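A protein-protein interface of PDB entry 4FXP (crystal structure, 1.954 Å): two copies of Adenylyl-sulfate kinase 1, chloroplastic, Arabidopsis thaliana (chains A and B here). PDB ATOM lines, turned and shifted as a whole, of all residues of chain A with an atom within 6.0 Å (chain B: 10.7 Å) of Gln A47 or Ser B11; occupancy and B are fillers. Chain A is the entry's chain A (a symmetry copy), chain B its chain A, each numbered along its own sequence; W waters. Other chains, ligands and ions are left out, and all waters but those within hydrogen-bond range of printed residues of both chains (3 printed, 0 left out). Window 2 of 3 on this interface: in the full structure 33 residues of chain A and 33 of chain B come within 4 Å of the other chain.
The side-chain amide nitrogen (NE2) of Gln A47 sits at hydrogen-bond distance from the side-chain hydroxyl (OG) of Ser B11 (2.9 Å).
The backbone carbonyl oxygen of Asp B16 is in hydrogen-bond range of the side-chain hydroxyl of Tyr A50, 2.6 Å away.
The side-chain sulfur of Cys A43 forms a disulfide with the side-chain sulfur of Cys B10 (2.0 Å).
The side-chain hydroxyl of Tyr A50 is in hydrogen-bond range of the guanidinium group of Arg B19, 3.0 Å away.
N of Glu B13 sits at hydrogen-bond distance from OD2 of Asp B16 (2.7 Å).
The side-chain carboxylate of Asp B16 lies within salt-bridge range of the guanidinium group of Arg B19 (3.0 Å).
The backbone carbonyl oxygen (O) of Val B12 sits at hydrogen-bond distance from the guanidinium group (NH1) of Arg B17 (3.4 Å).
Among the printed residues, pairs that only touch across the chains: Asn A46 with Val B12, Gln A47 with Val B12 and Tyr A50 with Leu B20.
Printed residues of chain B within 4 Å of Gln A47: Ser B11 and Val B12.
Printed residues of chain A within 4 Å of Ser B11: Gln A47.
No residue of chain B comes within 4 Å of Ala A44.
Printed residues of chain B within 4 Å of Asn A46: Val B12.
Met A48 touches none of the printed residues of chain B.
Printed residues of chain A within 4 Å of Leu B20: Tyr A50.
Printed residues of chain A within 4 Å of Val B12: Asn A46 (3.7 Å) and Gln A47 (3.7 Å).
Of the printed residues of chain A, Asp B16 touches Tyr A50.
Printed residues of chain A within 4 Å of Cys B10: Cys A43 (2.0 Å).
Of the printed residues of chain B, Cys A43 touches Cys B10 (2.0 Å).
Glu B13 touches none of the printed residues of chain A.
The nearest printed residue of chain A that does not touch Val B12 is Tyr A50 (4.03 Å).
Of the 11 printed residues of chain B, 6 touch a printed residue of chain A.
Printed residues of chain B that touch a printed residue of chain A: Cys B10, Ser B11, Val B12, Asp B16, Arg B19 and Leu B20.
Of the 11 printed residues of chain A, 4 touch a printed residue of chain B.
Printed residues of chain A that touch a printed residue of chain B: Cys A43, Asn A46, Gln A47 and Tyr A50.
Among the printed residues, no Asp or Glu carboxylate lies within 4 Å of a Lys or Arg side-chain nitrogen of the other chain.
No position is printed for both chains.
Water W1 lies within hydrogen-bond range of ND2 of Asn A46 (2.8 Å) and O of Val B12 (2.9 Å).
Water W3 lies within hydrogen-bond range of the side-chain amide oxygen (OD1) of Asn A46 and the guanidinium group (NH1) of Arg B17.
Water W2 lies within hydrogen-bond range of the side-chain sulfur (SG) of Cys A43 (3.2 Å) and the side-chain sulfur (SG) of Cys B10 (3.4 Å).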
ATOM      1  N   ALA A  42     -34.200  -5.361  -6.692  1.00  0.00           N
ATOM      2  CA  ALA A  42     -33.159  -4.560  -7.338  1.00  0.00           C
ATOM      3  C   ALA A  42     -31.853  -4.566  -6.542  1.00  0.00           C
ATOM      4  O   ALA A  42     -30.789  -4.762  -7.110  1.00  0.00           O
ATOM      5  CB  ALA A  42     -33.636  -3.116  -7.615  1.00  0.00           C
ATOM      6  N   CYS A  43     -31.940  -4.354  -5.231  1.00  0.00           N
ATOM      7  CA  CYS A  43     -30.750  -4.340  -4.375  1.00  0.00           C
ATOM      8  C   CYS A  43     -30.021  -5.690  -4.338  1.00  0.00           C
ATOM      9  O   CYS A  43     -28.787  -5.747  -4.392  1.00  0.00           O
ATOM     10  CB  CYS A  43     -31.112  -3.901  -2.947  1.00  0.00           C
ATOM     11  SG  CYS A  43     -31.546  -2.140  -2.779  1.00  0.00           S
ATOM     12  N   ALA A  44     -30.784  -6.772  -4.227  1.00  0.00           N
ATOM     13  CA  ALA A  44     -30.201  -8.115  -4.189  1.00  0.00           C
ATOM     14  C   ALA A  44     -29.493  -8.413  -5.505  1.00  0.00           C
ATOM     15  O   ALA A  44     -28.408  -8.974  -5.512  1.00  0.00           O
ATOM     16  CB  ALA A  44     -31.274  -9.175  -3.920  1.00  0.00           C
ATOM     17  N   LEU A  45     -30.134  -8.060  -6.614  1.00  0.00           N
ATOM     18  CA  LEU A  45     -29.566  -8.290  -7.935  1.00  0.00           C
ATOM     19  C   LEU A  45     -28.280  -7.474  -8.107  1.00  0.00           C
ATOM     20  O   LEU A  45     -27.259  -7.982  -8.556  1.00  0.00           O
ATOM     21  CB  LEU A  45     -30.601  -7.934  -9.005  1.00  0.00           C
ATOM     22  CG  LEU A  45     -30.209  -7.894 -10.477  1.00  0.00           C
ATOM     23  CD1 LEU A  45     -29.596  -9.221 -10.906  1.00  0.00           C
ATOM     24  CD2 LEU A  45     -31.439  -7.572 -11.329  1.00  0.00           C
ATOM     25  N   ASN A  46     -28.329  -6.210  -7.715  1.00  0.00           N
ATOM     26  CA  ASN A  46     -27.146  -5.335  -7.777  1.00  0.00           C
ATOM     27  C   ASN A  46     -25.961  -5.916  -7.001  1.00  0.00           C
ATOM     28  O   ASN A  46     -24.843  -6.009  -7.524  1.00  0.00           O
ATOM     29  CB  ASN A  46     -27.527  -3.957  -7.256  1.00  0.00           C
ATOM     30  CG  ASN A  46     -26.448  -2.899  -7.503  1.00  0.00           C
ATOM     31  OD1 ASN A  46     -25.452  -3.143  -8.172  1.00  0.00           O
ATOM     32  ND2 ASN A  46     -26.663  -1.724  -6.961  1.00  0.00           N
ATOM     33  N   GLN A  47     -26.218  -6.336  -5.764  1.00  0.00           N
ATOM     34  CA  GLN A  47     -25.185  -6.922  -4.913  1.00  0.00           C
ATOM     35  C   GLN A  47     -24.587  -8.159  -5.558  1.00  0.00           C
ATOM     36  O   GLN A  47     -23.369  -8.344  -5.589  1.00  0.00           O
ATOM     37  CB  GLN A  47     -25.766  -7.306  -3.546  1.00  0.00           C
ATOM     38  CG  GLN A  47     -26.317  -6.141  -2.736  1.00  0.00           C
ATOM     39  CD  GLN A  47     -26.990  -6.604  -1.448  1.00  0.00           C
ATOM     40  OE1 GLN A  47     -26.908  -7.777  -1.086  1.00  0.00           O
ATOM     41  NE2 GLN A  47     -27.661  -5.685  -0.754  1.00  0.00           N
ATOM     42  N   MET A  48     -25.467  -9.017  -6.065  1.00  0.00           N
ATOM     43  CA  MET A  48     -25.061 -10.270  -6.678  1.00  0.00           C
ATOM     44  C   MET A  48     -24.223 -10.049  -7.940  1.00  0.00           C
ATOM     45  O   MET A  48     -23.215 -10.725  -8.167  1.00  0.00           O
ATOM     46  CB  MET A  48     -26.328 -11.064  -7.023  1.00  0.00           C
ATOM     47  CG  MET A  48     -26.125 -12.503  -7.359  1.00  0.00           C
ATOM     48  SD  MET A  48     -27.756 -13.276  -7.439  1.00  0.00           S
ATOM     49  CE  MET A  48     -28.293 -13.085  -5.756  1.00  0.00           C
ATOM     50  N   LEU A  49     -24.652  -9.105  -8.768  1.00  0.00           N
ATOM     51  CA  LEU A  49     -23.901  -8.765  -9.979  1.00  0.00           C
ATOM     52  C   LEU A  49     -22.577  -8.093  -9.641  1.00  0.00           C
ATOM     53  O   LEU A  49     -21.547  -8.405 -10.239  1.00  0.00           O
ATOM     54  CB  LEU A  49     -24.735  -7.884 -10.905  1.00  0.00           C
ATOM     55  CG  LEU A  49     -25.853  -8.669 -11.608  1.00  0.00           C
ATOM     56  CD1 LEU A  49     -26.793  -7.741 -12.343  1.00  0.00           C
ATOM     57  CD2 LEU A  49     -25.252  -9.695 -12.555  1.00  0.00           C
ATOM     58  N   TYR A  50     -22.590  -7.192  -8.665  1.00  0.00           N
ATOM     59  CA  TYR A  50     -21.335  -6.576  -8.227  1.00  0.00           C
ATOM     60  C   TYR A  50     -20.315  -7.641  -7.818  1.00  0.00           C
ATOM     61  O   TYR A  50     -19.153  -7.600  -8.234  1.00  0.00           O
ATOM     62  CB  TYR A  50     -21.551  -5.607  -7.070  1.00  0.00           C
ATOM     63  CG  TYR A  50     -20.256  -4.890  -6.723  1.00  0.00           C
ATOM     64  CD1 TYR A  50     -19.850  -3.780  -7.446  1.00  0.00           C
ATOM     65  CD2 TYR A  50     -19.416  -5.366  -5.715  1.00  0.00           C
ATOM     66  CE1 TYR A  50     -18.649  -3.125  -7.155  1.00  0.00           C
ATOM     67  CE2 TYR A  50     -18.205  -4.725  -5.423  1.00  0.00           C
ATOM     68  CZ  TYR A  50     -17.833  -3.605  -6.148  1.00  0.00           C
ATOM     69  OH  TYR A  50     -16.635  -2.949  -5.873  1.00  0.00           O
ATOM     70  N   GLN A  51     -20.744  -8.604  -7.008  1.00  0.00           N
ATOM     71  CA  GLN A  51     -19.822  -9.630  -6.526  1.00  0.00           C
ATOM     72  C   GLN A  51     -19.228 -10.444  -7.685  1.00  0.00           C
ATOM     73  O   GLN A  51     -18.106 -10.941  -7.588  1.00  0.00           O
ATOM     74  CB  GLN A  51     -20.502 -10.526  -5.481  1.00  0.00           C
ATOM     75  CG  GLN A  51     -19.592 -11.580  -4.859  1.00  0.00           C
ATOM     76  CD  GLN A  51     -20.168 -12.156  -3.562  1.00  0.00           C
ATOM     77  OE1 GLN A  51     -20.970 -11.508  -2.889  1.00  0.00           O
ATOM     78  NE2 GLN A  51     -19.752 -13.373  -3.208  1.00  0.00           N
ATOM     79  N   LYS A  52     -19.973 -10.547  -8.784  1.00  0.00           N
ATOM     80  CA  LYS A  52     -19.493 -11.194 -10.012  1.00  0.00           C
ATOM     81  C   LYS A  52     -18.626 -10.267 -10.891  1.00  0.00           C
ATOM     82  O   LYS A  52     -18.144 -10.677 -11.949  1.00  0.00           O
ATOM     83  CB  LYS A  52     -20.675 -11.696 -10.844  1.00  0.00           C
ATOM     84  CG  LYS A  52     -21.427 -12.889 -10.239  1.00  0.00           C
ATOM     85  CD  LYS A  52     -22.532 -13.359 -11.189  1.00  0.00           C
ATOM     86  CE  LYS A  52     -22.554 -14.880 -11.298  1.00  0.00           C
ATOM     87  NZ  LYS A  52     -22.806 -15.524  -9.976  1.00  0.00           N
ATOM     88  N   GLU B   9     -32.053   2.483  -0.100  1.00  0.00           N
ATOM     89  CA  GLU B   9     -30.604   2.428  -0.250  1.00  0.00           C
ATOM     90  C   GLU B   9     -30.099   0.989  -0.298  1.00  0.00           C
ATOM     91  O   GLU B   9     -30.415   0.175   0.572  1.00  0.00           O
ATOM     92  CB  GLU B   9     -29.922   3.185   0.891  1.00  0.00           C
ATOM     93  CG  GLU B   9     -30.165   4.687   0.874  1.00  0.00           C
ATOM     94  CD  GLU B   9     -29.533   5.391   2.059  1.00  0.00           C
ATOM     95  OE1 GLU B   9     -29.073   4.696   2.989  1.00  0.00           O
ATOM     96  OE2 GLU B   9     -29.500   6.639   2.062  1.00  0.00           O
ATOM     97  N   CYS B  10     -29.308   0.686  -1.322  1.00  0.00           N
ATOM     98  CA  CYS B  10     -28.716  -0.637  -1.466  1.00  0.00           C
ATOM     99  C   CYS B  10     -27.323  -0.660  -0.860  1.00  0.00           C
ATOM    100  O   CYS B  10     -26.705   0.387  -0.654  1.00  0.00           O
ATOM    101  CB  CYS B  10     -28.644  -1.017  -2.945  1.00  0.00           C
ATOM    102  SG  CYS B  10     -30.236  -0.941  -3.775  1.00  0.00           S
ATOM    103  N   SER B  11     -26.822  -1.857  -0.584  1.00  0.00           N
ATOM    104  CA  SER B  11     -25.481  -1.992  -0.017  1.00  0.00           C
ATOM    105  C   SER B  11     -24.365  -1.584  -0.992  1.00  0.00           C
ATOM    106  O   SER B  11     -23.290  -1.189  -0.557  1.00  0.00           O
ATOM    107  CB  SER B  11     -25.241  -3.420   0.466  1.00  0.00           C
ATOM    108  OG  SER B  11     -25.150  -4.308  -0.630  1.00  0.00           O
ATOM    109  N   VAL B  12     -24.605  -1.690  -2.299  1.00  0.00           N
ATOM    110  CA  VAL B  12     -23.572  -1.313  -3.274  1.00  0.00           C
ATOM    111  C   VAL B  12     -23.466   0.207  -3.409  1.00  0.00           C
ATOM    112  O   VAL B  12     -24.407   0.867  -3.851  1.00  0.00           O
ATOM    113  CB  VAL B  12     -23.799  -1.945  -4.661  1.00  0.00           C
ATOM    114  CG1 VAL B  12     -22.673  -1.527  -5.609  1.00  0.00           C
ATOM    115  CG2 VAL B  12     -23.847  -3.466  -4.544  1.00  0.00           C
ATOM    116  N   GLU B  13     -22.307   0.748  -3.041  1.00  0.00           N
ATOM    117  CA  GLU B  13     -22.091   2.202  -2.995  1.00  0.00           C
ATOM    118  C   GLU B  13     -21.311   2.757  -4.188  1.00  0.00           C
ATOM    119  O   GLU B  13     -20.724   2.016  -4.966  1.00  0.00           O
ATOM    120  CB  GLU B  13     -21.323   2.568  -1.723  1.00  0.00           C
ATOM    121  CG  GLU B  13     -22.050   2.268  -0.441  1.00  0.00           C
ATOM    122  CD  GLU B  13     -21.259   2.699   0.782  1.00  0.00           C
ATOM    123  OE1 GLU B  13     -21.544   2.185   1.880  1.00  0.00           O
ATOM    124  OE2 GLU B  13     -20.361   3.558   0.648  1.00  0.00           O
ATOM    125  N   LYS B  14     -21.295   4.079  -4.318  1.00  0.00           N
ATOM    126  CA  LYS B  14     -20.517   4.721  -5.372  1.00  0.00           C
ATOM    127  C   LYS B  14     -19.049   4.300  -5.290  1.00  0.00           C
ATOM    128  O   LYS B  14     -18.433   4.004  -6.314  1.00  0.00           O
ATOM    129  CB  LYS B  14     -20.657   6.244  -5.286  1.00  0.00           C
ATOM    130  CG  LYS B  14     -19.803   7.048  -6.279  1.00  0.00           C
ATOM    131  CD  LYS B  14     -20.264   8.511  -6.256  1.00  0.00           C
ATOM    132  CE  LYS B  14     -19.247   9.449  -6.876  1.00  0.00           C
ATOM    133  NZ  LYS B  14     -18.338  10.007  -5.836  1.00  0.00           N
ATOM    134  N   VAL B  15     -18.492   4.254  -4.082  1.00  0.00           N
ATOM    135  CA  VAL B  15     -17.083   3.878  -3.944  1.00  0.00           C
ATOM    136  C   VAL B  15     -16.826   2.443  -4.394  1.00  0.00           C
ATOM    137  O   VAL B  15     -15.723   2.112  -4.819  1.00  0.00           O
ATOM    138  CB  VAL B  15     -16.542   4.094  -2.508  1.00  0.00           C
ATOM    139  CG1 VAL B  15     -16.293   5.577  -2.252  1.00  0.00           C
ATOM    140  CG2 VAL B  15     -17.486   3.512  -1.469  1.00  0.00           C
ATOM    141  N   ASP B  16     -17.848   1.594  -4.293  1.00  0.00           N
ATOM    142  CA  ASP B  16     -17.753   0.216  -4.788  1.00  0.00           C
ATOM    143  C   ASP B  16     -17.674   0.201  -6.313  1.00  0.00           C
ATOM    144  O   ASP B  16     -16.881  -0.540  -6.911  1.00  0.00           O
ATOM    145  CB  ASP B  16     -18.977  -0.593  -4.331  1.00  0.00           C
ATOM    146  CG  ASP B  16     -19.019  -0.778  -2.821  1.00  0.00           C
ATOM    147  OD1 ASP B  16     -17.971  -1.123  -2.231  1.00  0.00           O
ATOM    148  OD2 ASP B  16     -20.097  -0.564  -2.228  1.00  0.00           O
ATOM    149  N   ARG B  17     -18.506   1.015  -6.949  1.00  0.00           N
ATOM    150  CA  ARG B  17     -18.469   1.106  -8.401  1.00  0.00           C
ATOM    151  C   ARG B  17     -17.131   1.690  -8.857  1.00  0.00           C
ATOM    152  O   ARG B  17     -16.565   1.260  -9.863  1.00  0.00           O
ATOM    153  CB  ARG B  17     -19.645   1.934  -8.924  1.00  0.00           C
ATOM    154  CG  ARG B  17     -21.002   1.196  -8.751  1.00  0.00           C
ATOM    155  CD  ARG B  17     -22.182   1.988  -9.292  1.00  0.00           C
ATOM    156  NE  ARG B  17     -22.554   3.138  -8.464  1.00  0.00           N
ATOM    157  CZ  ARG B  17     -23.382   3.078  -7.423  1.00  0.00           C
ATOM    158  NH1 ARG B  17     -23.908   1.919  -7.065  1.00  0.00           N
ATOM    159  NH2 ARG B  17     -23.684   4.176  -6.734  1.00  0.00           N
ATOM    160  N   ARG B  19     -14.252   1.499  -7.268  1.00  0.00           N
ATOM    161  CA  ARG B  19     -13.283   0.442  -7.018  1.00  0.00           C
ATOM    162  C   ARG B  19     -13.273  -0.559  -8.180  1.00  0.00           C
ATOM    163  O   ARG B  19     -12.218  -1.007  -8.644  1.00  0.00           O
ATOM    164  CB  ARG B  19     -13.648  -0.263  -5.702  1.00  0.00           C
ATOM    165  CG  ARG B  19     -12.509  -0.957  -4.999  1.00  0.00           C
ATOM    166  CD  ARG B  19     -12.810  -1.097  -3.503  1.00  0.00           C
ATOM    167  NE  ARG B  19     -14.182  -1.528  -3.228  1.00  0.00           N
ATOM    168  CZ  ARG B  19     -14.577  -2.793  -3.247  1.00  0.00           C
ATOM    169  NH1 ARG B  19     -13.710  -3.752  -3.552  1.00  0.00           N
ATOM    170  NH2 ARG B  19     -15.838  -3.105  -2.968  1.00  0.00           N
ATOM    171  N   LEU B  20     -14.458  -0.910  -8.652  1.00  0.00           N
ATOM    172  CA  LEU B  20     -14.584  -1.844  -9.760  1.00  0.00           C
ATOM    173  C   LEU B  20     -13.972  -1.261 -11.047  1.00  0.00           C
ATOM    174  O   LEU B  20     -13.296  -1.967 -11.796  1.00  0.00           O
ATOM    175  CB  LEU B  20     -16.060  -2.190  -9.981  1.00  0.00           C
ATOM    176  CG  LEU B  20     -16.404  -3.172 -11.094  1.00  0.00           C
ATOM    177  CD1 LEU B  20     -15.631  -4.470 -10.923  1.00  0.00           C
ATOM    178  CD2 LEU B  20     -17.901  -3.455 -11.077  1.00  0.00           C
HETATM  179  O   HOH W   1     -26.849   0.607  -5.475  1.00  0.00           O
HETATM  180  O   HOH W   2     -33.460  -0.511  -4.807  1.00  0.00           O
HETATM  181  O   HOH W   3     -23.958  -0.708  -8.468  1.00  0.00           O
